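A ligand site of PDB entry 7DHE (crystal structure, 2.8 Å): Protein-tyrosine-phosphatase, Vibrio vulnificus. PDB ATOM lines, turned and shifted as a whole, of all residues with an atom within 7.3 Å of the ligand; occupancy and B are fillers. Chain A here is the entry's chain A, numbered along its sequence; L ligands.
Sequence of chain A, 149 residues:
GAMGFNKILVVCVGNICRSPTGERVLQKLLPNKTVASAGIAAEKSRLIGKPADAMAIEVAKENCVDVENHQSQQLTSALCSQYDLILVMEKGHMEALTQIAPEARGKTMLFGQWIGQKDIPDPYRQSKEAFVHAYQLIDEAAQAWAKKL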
ATOM      1  N   VAL A  11      18.317   9.781  21.443  1.00  0.00           N
ATOM      2  CA  VAL A  11      18.396  11.007  20.652  1.00  0.00           C
ATOM      3  C   VAL A  11      17.915  10.798  19.236  1.00  0.00           C
ATOM      4  O   VAL A  11      18.292   9.817  18.586  1.00  0.00           O
ATOM      5  CB  VAL A  11      19.867  11.576  20.693  1.00  0.00           C
ATOM      6  CG1 VAL A  11      20.055  12.754  19.740  1.00  0.00           C
ATOM      7  CG2 VAL A  11      20.300  11.945  22.111  1.00  0.00           C
ATOM      8  N   CYS A  12      17.072  11.740  18.751  1.00  0.00           N
ATOM      9  CA  CYS A  12      16.638  11.892  17.380  1.00  0.00           C
ATOM     10  C   CYS A  12      16.628  13.371  17.031  1.00  0.00           C
ATOM     11  O   CYS A  12      17.414  14.116  17.628  1.00  0.00           O
ATOM     12  CB  CYS A  12      15.336  11.179  17.065  1.00  0.00           C
ATOM     13  SG  CYS A  12      13.834  11.985  17.680  1.00  0.00           S
ATOM     14  N   VAL A  13      15.835  13.820  16.046  1.00  0.00           N
ATOM     15  CA  VAL A  13      15.964  15.230  15.679  1.00  0.00           C
ATOM     16  C   VAL A  13      14.848  16.118  16.296  1.00  0.00           C
ATOM     17  O   VAL A  13      15.177  17.213  16.766  1.00  0.00           O
ATOM     18  CB  VAL A  13      16.228  15.520  14.182  1.00  0.00           C
ATOM     19  CG1 VAL A  13      16.469  14.293  13.322  1.00  0.00           C
ATOM     20  CG2 VAL A  13      15.296  16.566  13.567  1.00  0.00           C
ATOM     21  N   GLY A  14      13.599  15.665  16.312  1.00  0.00           N
ATOM     22  CA  GLY A  14      12.581  16.507  16.891  1.00  0.00           C
ATOM     23  C   GLY A  14      12.201  16.180  18.305  1.00  0.00           C
ATOM     24  O   GLY A  14      11.566  17.004  18.977  1.00  0.00           O
ATOM     25  N   ASN A  15      12.532  14.959  18.764  1.00  0.00           N
ATOM     26  CA  ASN A  15      12.153  14.452  20.099  1.00  0.00           C
ATOM     27  C   ASN A  15      10.624  14.395  20.269  1.00  0.00           C
ATOM     28  O   ASN A  15      10.105  14.676  21.338  1.00  0.00           O
ATOM     29  CB  ASN A  15      12.834  15.208  21.230  1.00  0.00           C
ATOM     30  CG  ASN A  15      12.774  14.552  22.586  1.00  0.00           C
ATOM     31  OD1 ASN A  15      12.595  15.196  23.640  1.00  0.00           O
ATOM     32  ND2 ASN A  15      12.948  13.241  22.608  1.00  0.00           N
ATOM     33  N   ILE A  16       9.912  14.003  19.209  1.00  0.00           N
ATOM     34  CA  ILE A  16       8.460  13.860  19.258  1.00  0.00           C
ATOM     35  C   ILE A  16       8.010  12.478  18.767  1.00  0.00           C
ATOM     36  O   ILE A  16       6.894  12.047  19.078  1.00  0.00           O
ATOM     37  CB  ILE A  16       7.701  15.030  18.531  1.00  0.00           C
ATOM     38  CG1 ILE A  16       8.205  15.192  17.057  1.00  0.00           C
ATOM     39  CG2 ILE A  16       7.837  16.333  19.328  1.00  0.00           C
ATOM     40  CD1 ILE A  16       7.345  15.908  16.184  1.00  0.00           C
ATOM     41  N   CYS A  17       8.831  11.802  17.964  1.00  0.00           N
ATOM     42  CA  CYS A  17       8.465  10.492  17.401  1.00  0.00           C
ATOM     43  C   CYS A  17       9.355   9.341  17.896  1.00  0.00           C
ATOM     44  O   CYS A  17       8.981   8.606  18.808  1.00  0.00           O
ATOM     45  CB  CYS A  17       8.409  10.533  15.877  1.00  0.00           C
ATOM     46  SG  CYS A  17       7.033  11.486  15.214  1.00  0.00           S
ATOM     47  N   ARG A  18      10.487   9.176  17.255  1.00  0.00           N
ATOM     48  CA  ARG A  18      11.341   8.030  17.537  1.00  0.00           C
ATOM     49  C   ARG A  18      11.947   8.040  18.927  1.00  0.00           C
ATOM     50  O   ARG A  18      11.836   7.042  19.641  1.00  0.00           O
ATOM     51  CB  ARG A  18      12.416   7.879  16.451  1.00  0.00           C
ATOM     52  CG  ARG A  18      11.846   7.607  15.039  1.00  0.00           C
ATOM     53  CD  ARG A  18      12.908   7.820  14.012  1.00  0.00           C
ATOM     54  NE  ARG A  18      13.234   9.218  13.922  1.00  0.00           N
ATOM     55  CZ  ARG A  18      14.224   9.705  13.186  1.00  0.00           C
ATOM     56  NH1 ARG A  18      14.971   8.904  12.458  1.00  0.00           N
ATOM     57  NH2 ARG A  18      14.464  11.003  13.180  1.00  0.00           N
ATOM     58  N   SER A  19      12.613   9.136  19.296  1.00  0.00           N
ATOM     59  CA  SER A  19      13.326   9.199  20.564  1.00  0.00           C
ATOM     60  C   SER A  19      12.399   9.084  21.794  1.00  0.00           C
ATOM     61  O   SER A  19      12.736   8.297  22.691  1.00  0.00           O
ATOM     62  CB  SER A  19      14.242  10.408  20.645  1.00  0.00           C
ATOM     63  OG  SER A  19      13.605  11.648  20.409  1.00  0.00           O
ATOM     64  N   PRO A  20      11.206   9.722  21.872  1.00  0.00           N
ATOM     65  CA  PRO A  20      10.355   9.438  23.026  1.00  0.00           C
ATOM     66  C   PRO A  20       9.899   7.957  23.050  1.00  0.00           C
ATOM     67  O   PRO A  20       9.782   7.373  24.139  1.00  0.00           O
ATOM     68  CB  PRO A  20       9.194  10.407  22.864  1.00  0.00           C
ATOM     69  CG  PRO A  20       9.228  10.839  21.490  1.00  0.00           C
ATOM     70  CD  PRO A  20      10.610  10.767  21.017  1.00  0.00           C
ATOM     71  N   ALA A  38      16.110  13.342  23.881  1.00  0.00           N
ATOM     72  CA  ALA A  38      16.280  14.713  23.405  1.00  0.00           C
ATOM     73  C   ALA A  38      16.393  14.760  21.883  1.00  0.00           C
ATOM     74  O   ALA A  38      16.681  13.738  21.238  1.00  0.00           O
ATOM     75  CB  ALA A  38      17.484  15.358  24.046  1.00  0.00           C
ATOM     76  N   GLY A  39      16.139  15.947  21.317  1.00  0.00           N
ATOM     77  CA  GLY A  39      16.189  16.191  19.878  1.00  0.00           C
ATOM     78  C   GLY A  39      17.281  17.146  19.464  1.00  0.00           C
ATOM     79  O   GLY A  39      17.453  18.204  20.076  1.00  0.00           O
ATOM     80  N   ALA A  41      17.411  18.989  16.782  1.00  0.00           N
ATOM     81  CA  ALA A  41      16.864  20.229  16.246  1.00  0.00           C
ATOM     82  C   ALA A  41      15.500  20.568  16.837  1.00  0.00           C
ATOM     83  O   ALA A  41      14.702  21.241  16.182  1.00  0.00           O
ATOM     84  CB  ALA A  41      16.790  20.157  14.727  1.00  0.00           C
ATOM     85  N   ALA A  42      15.262  20.148  18.101  1.00  0.00           N
ATOM     86  CA  ALA A  42      13.986  20.426  18.754  1.00  0.00           C
ATOM     87  C   ALA A  42      13.711  21.940  18.850  1.00  0.00           C
ATOM     88  O   ALA A  42      12.596  22.386  18.602  1.00  0.00           O
ATOM     89  CB  ALA A  42      13.936  19.770  20.127  1.00  0.00           C
ATOM     90  N   SER A  45      13.184  23.559  15.339  1.00  0.00           N
ATOM     91  CA  SER A  45      11.906  23.089  14.832  1.00  0.00           C
ATOM     92  C   SER A  45      10.735  23.658  15.621  1.00  0.00           C
ATOM     93  O   SER A  45       9.586  23.387  15.280  1.00  0.00           O
ATOM     94  CB  SER A  45      11.858  21.564  14.852  1.00  0.00           C
ATOM     95  OG  SER A  45      12.923  20.992  14.104  1.00  0.00           O
ATOM     96  N   LEU A  47       9.762  22.849  18.597  1.00  0.00           N
ATOM     97  CA  LEU A  47       9.081  21.718  19.208  1.00  0.00           C
ATOM     98  C   LEU A  47       9.243  21.573  20.710  1.00  0.00           C
ATOM     99  O   LEU A  47       8.609  20.708  21.305  1.00  0.00           O
ATOM    100  CB  LEU A  47       9.511  20.417  18.523  1.00  0.00           C
ATOM    101  CG  LEU A  47       9.099  20.238  17.078  1.00  0.00           C
ATOM    102  CD1 LEU A  47       9.703  18.967  16.545  1.00  0.00           C
ATOM    103  CD2 LEU A  47       7.600  20.221  16.914  1.00  0.00           C
ATOM    104  N   ASP A  53       4.183  12.754  19.302  1.00  0.00           N
ATOM    105  CA  ASP A  53       3.184  12.690  18.244  1.00  0.00           C
ATOM    106  C   ASP A  53       2.039  11.708  18.630  1.00  0.00           C
ATOM    107  O   ASP A  53       2.313  10.605  19.141  1.00  0.00           O
ATOM    108  CB  ASP A  53       3.871  12.230  16.970  1.00  0.00           C
ATOM    109  CG  ASP A  53       2.949  12.240  15.787  1.00  0.00           C
ATOM    110  OD1 ASP A  53       2.971  13.227  15.020  1.00  0.00           O
ATOM    111  OD2 ASP A  53       2.202  11.263  15.613  1.00  0.00           O
ATOM    112  N   SER A  72       9.088  17.405  24.547  1.00  0.00           N
ATOM    113  CA  SER A  72      10.261  17.477  23.692  1.00  0.00           C
ATOM    114  C   SER A  72      11.285  18.441  24.259  1.00  0.00           C
ATOM    115  O   SER A  72      10.938  19.535  24.743  1.00  0.00           O
ATOM    116  CB  SER A  72       9.878  17.928  22.281  1.00  0.00           C
ATOM    117  OG  SER A  72      11.036  18.165  21.489  1.00  0.00           O
ATOM    118  N   MET A  89      19.224   7.620  16.697  1.00  0.00           N
ATOM    119  CA  MET A  89      18.299   6.841  15.867  1.00  0.00           C
ATOM    120  C   MET A  89      18.855   6.568  14.505  1.00  0.00           C
ATOM    121  O   MET A  89      18.516   5.542  13.915  1.00  0.00           O
ATOM    122  CB  MET A  89      16.932   7.521  15.783  1.00  0.00           C
ATOM    123  CG  MET A  89      16.099   7.362  17.036  1.00  0.00           C
ATOM    124  SD  MET A  89      15.608   5.641  17.260  1.00  0.00           S
ATOM    125  CE  MET A  89      15.013   5.673  18.927  1.00  0.00           C
ATOM    126  N   GLU A  90      19.710   7.458  13.999  1.00  0.00           N
ATOM    127  CA  GLU A  90      20.386   7.322  12.699  1.00  0.00           C
ATOM    128  C   GLU A  90      21.885   7.586  12.838  1.00  0.00           C
ATOM    129  O   GLU A  90      22.298   8.432  13.633  1.00  0.00           O
ATOM    130  CB  GLU A  90      19.811   8.327  11.677  1.00  0.00           C
ATOM    131  CG  GLU A  90      18.376   8.087  11.265  1.00  0.00           C
ATOM    132  CD  GLU A  90      17.848   9.097  10.261  1.00  0.00           C
ATOM    133  OE1 GLU A  90      18.629   9.544   9.393  1.00  0.00           O
ATOM    134  OE2 GLU A  90      16.653   9.448  10.340  1.00  0.00           O
ATOM    135  N   HIS A  93      23.020  11.122  12.597  1.00  0.00           N
ATOM    136  CA  HIS A  93      22.834  11.946  13.792  1.00  0.00           C
ATOM    137  C   HIS A  93      24.127  12.164  14.571  1.00  0.00           C
ATOM    138  O   HIS A  93      24.230  13.119  15.337  1.00  0.00           O
ATOM    139  CB  HIS A  93      21.752  11.341  14.696  1.00  0.00           C
ATOM    140  CG  HIS A  93      20.375  11.314  14.094  1.00  0.00           C
ATOM    141  ND1 HIS A  93      19.362  10.545  14.644  1.00  0.00           N
ATOM    142  CD2 HIS A  93      19.885  11.957  13.004  1.00  0.00           C
ATOM    143  CE1 HIS A  93      18.305  10.737  13.880  1.00  0.00           C
ATOM    144  NE2 HIS A  93      18.575  11.569  12.872  1.00  0.00           N
ATOM    145  N   ILE A 120      16.801   3.887  12.180  1.00  0.00           N
ATOM    146  CA  ILE A 120      15.376   3.832  12.416  1.00  0.00           C
ATOM    147  C   ILE A 120      14.739   5.014  11.686  1.00  0.00           C
ATOM    148  O   ILE A 120      15.030   6.166  11.993  1.00  0.00           O
ATOM    149  CB  ILE A 120      15.038   3.716  13.908  1.00  0.00           C
ATOM    150  CG1 ILE A 120      15.523   2.340  14.393  1.00  0.00           C
ATOM    151  CG2 ILE A 120      13.524   3.886  14.103  1.00  0.00           C
ATOM    152  CD1 ILE A 120      15.573   2.114  15.773  1.00  0.00           C
ATOM    153  N   PRO A 121      13.922   4.735  10.660  1.00  0.00           N
ATOM    154  CA  PRO A 121      13.370   5.824   9.838  1.00  0.00           C
ATOM    155  C   PRO A 121      12.349   6.709  10.526  1.00  0.00           C
ATOM    156  O   PRO A 121      11.549   6.235  11.310  1.00  0.00           O
ATOM    157  CB  PRO A 121      12.757   5.081   8.655  1.00  0.00           C
ATOM    158  CG  PRO A 121      12.301   3.760   9.285  1.00  0.00           C
ATOM    159  CD  PRO A 121      13.452   3.419  10.184  1.00  0.00           C
ATOM    160  N   ASP A 122      12.382   7.967  10.211  1.00  0.00           N
ATOM    161  CA  ASP A 122      11.454   8.953  10.717  1.00  0.00           C
ATOM    162  C   ASP A 122      10.029   8.730  10.159  1.00  0.00           C
ATOM    163  O   ASP A 122       9.822   8.832   8.942  1.00  0.00           O
ATOM    164  CB  ASP A 122      11.967  10.341  10.349  1.00  0.00           C
ATOM    165  CG  ASP A 122      11.171  11.463  10.933  1.00  0.00           C
ATOM    166  OD1 ASP A 122      10.302  11.186  11.792  1.00  0.00           O
ATOM    167  OD2 ASP A 122      11.406  12.618  10.513  1.00  0.00           O
ATOM    168  N   PRO A 123       9.031   8.512  11.042  1.00  0.00           N
ATOM    169  CA  PRO A 123       7.650   8.367  10.554  1.00  0.00           C
ATOM    170  C   PRO A 123       6.850   9.690  10.470  1.00  0.00           C
ATOM    171  O   PRO A 123       5.694   9.692  10.051  1.00  0.00           O
ATOM    172  CB  PRO A 123       7.033   7.478  11.607  1.00  0.00           C
ATOM    173  CG  PRO A 123       7.723   7.894  12.881  1.00  0.00           C
ATOM    174  CD  PRO A 123       9.107   8.349  12.513  1.00  0.00           C
ATOM    175  N   TYR A 124       7.461  10.803  10.920  1.00  0.00           N
ATOM    176  CA  TYR A 124       6.777  12.074  11.021  1.00  0.00           C
ATOM    177  C   TYR A 124       6.140  12.502   9.717  1.00  0.00           C
ATOM    178  O   TYR A 124       6.753  12.330   8.654  1.00  0.00           O
ATOM    179  CB  TYR A 124       7.695  13.143  11.611  1.00  0.00           C
ATOM    180  CG  TYR A 124       6.979  14.396  12.046  1.00  0.00           C
ATOM    181  CD1 TYR A 124       5.954  14.348  13.000  1.00  0.00           C
ATOM    182  CD2 TYR A 124       7.322  15.634  11.517  1.00  0.00           C
ATOM    183  CE1 TYR A 124       5.273  15.510  13.374  1.00  0.00           C
ATOM    184  CE2 TYR A 124       6.642  16.796  11.891  1.00  0.00           C
ATOM    185  CZ  TYR A 124       5.642  16.735  12.852  1.00  0.00           C
ATOM    186  OH  TYR A 124       4.959  17.861  13.227  1.00  0.00           O
ATOM    187  N   ARG A 125       4.900  13.027   9.795  1.00  0.00           N
ATOM    188  CA  ARG A 125       4.086  13.516   8.661  1.00  0.00           C
ATOM    189  C   ARG A 125       3.515  12.389   7.810  1.00  0.00           C
ATOM    190  O   ARG A 125       2.889  12.663   6.786  1.00  0.00           O
ATOM    191  CB  ARG A 125       4.844  14.544   7.798  1.00  0.00           C
ATOM    192  CG  ARG A 125       5.108  15.846   8.493  1.00  0.00           C
ATOM    193  CD  ARG A 125       5.936  16.784   7.654  1.00  0.00           C
ATOM    194  NE  ARG A 125       7.270  16.874   8.249  1.00  0.00           N
ATOM    195  CZ  ARG A 125       7.709  17.908   8.954  1.00  0.00           C
ATOM    196  NH1 ARG A 125       8.926  17.874   9.487  1.00  0.00           N
ATOM    197  NH2 ARG A 125       6.945  18.967   9.141  1.00  0.00           N
ATOM    198  N   PHE A 131       4.440   4.708  11.544  1.00  0.00           N
ATOM    199  CA  PHE A 131       4.690   4.702  12.986  1.00  0.00           C
ATOM    200  C   PHE A 131       4.793   3.261  13.491  1.00  0.00           C
ATOM    201  O   PHE A 131       5.599   2.977  14.405  1.00  0.00           O
ATOM    202  CB  PHE A 131       3.591   5.477  13.693  1.00  0.00           C
ATOM    203  CG  PHE A 131       3.753   6.965  13.555  1.00  0.00           C
ATOM    204  CD1 PHE A 131       4.399   7.705  14.543  1.00  0.00           C
ATOM    205  CD2 PHE A 131       3.250   7.645  12.439  1.00  0.00           C
ATOM    206  CE1 PHE A 131       4.551   9.085  14.407  1.00  0.00           C
ATOM    207  CE2 PHE A 131       3.415   9.029  12.307  1.00  0.00           C
ATOM    208  CZ  PHE A 131       4.061   9.747  13.293  1.00  0.00           C
HETATM  209  C1  LIG L   1      10.386  15.825  14.261  1.00  0.00           C
HETATM  210  C2  LIG L   1      10.764  17.085  13.817  1.00  0.00           C
HETATM  211  C3  LIG L   1      11.437  17.221  12.626  1.00  0.00           C
HETATM  212  C4  LIG L   1      11.751  16.106  11.879  1.00  0.00           C
HETATM  213  C5  LIG L   1      11.386  14.849  12.327  1.00  0.00           C
HETATM  214  C6  LIG L   1      10.699  14.681  13.526  1.00  0.00           C
HETATM  215  C7  LIG L   1      10.334  13.306  14.027  1.00  0.00           C
HETATM  216  P1  LIG L   1      11.604  12.557  15.046  1.00  0.00           P
HETATM  217  O1  LIG L   1      11.330  11.034  15.134  1.00  0.00           O
HETATM  218  O2  LIG L   1      11.388  13.122  16.471  1.00  0.00           O
HETATM  219  O3  LIG L   1      12.970  12.895  14.519  1.00  0.00           O
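O3 of the ligand sits at hydrogen-bond distance from N of Gly 14 (3.4 Å).
O2 of the ligand sits at hydrogen-bond distance from N of Asn 15 (3.2 Å).
The guanidinium group (NH2) of Arg 18 is in salt-bridge range of an oxygen (O3) of the ligand (2.8 Å).
An oxygen (O3) of the ligand is in hydrogen-bond range of the backbone NH of Val 13 (3.4 Å).
An oxygen (O2) of the ligand lies within hydrogen-bond range of the backbone NH (N) of Cys 17, at 3.2 Å.
An oxygen (O1) of the ligand lies within hydrogen-bond range of the backbone NH (N) of Arg 18 (2.9 Å).
N of Ile 16 sits at hydrogen-bond distance from O2 of the ligand (3.2 Å).
SG of Cys 12 lies within hydrogen-bond range of O2 of the ligand, 3.0 Å away.
The backbone NH (N) of Ala 42 is in hydrogen-bond range of the backbone carbonyl oxygen (O) of Val 13 (3.2 Å).
O of Val 13 sits at hydrogen-bond distance from N of Ala 41 (2.9 Å).
The guanidinium group (NH1) of Arg 18 sits at hydrogen-bond distance from the backbone carbonyl oxygen (O) of Ile 120, 2.8 Å away.
The backbone carbonyl oxygen of Ile 16 is in hydrogen-bond range of the backbone NH of Asp 53.
N of Cys 12 lies within hydrogen-bond range of O of Ala 38 (3.2 Å).
The side-chain hydroxyl of Ser 19 sits at hydrogen-bond distance from the side-chain amide nitrogen of Asn 15 (2.8 Å).
N of Asn 15 sits at hydrogen-bond distance from SG of Cys 12, at 3.4 Å.
The side-chain carboxylate of Asp 122 sits at hydrogen-bond distance from the backbone NH of Tyr 124 (3.0 Å).
O1 of the ligand lies close to OD1 of Asp 122.
Leu 47 touches the ligand.
Tyr 124 touches the ligand (CB to C7, 3.6 Å).
Hydrophobic or aromatic side chains within 4 Å of the ligand: Val 13, Ile 16, Leu 47 and Tyr 124.
Ten residues have an atom within 4 Å of the ligand: Cys 12, Val 13, Gly 14, Asn 15, Ile 16, Cys 17, Arg 18, Leu 47, Asp 122 and Tyr 124.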
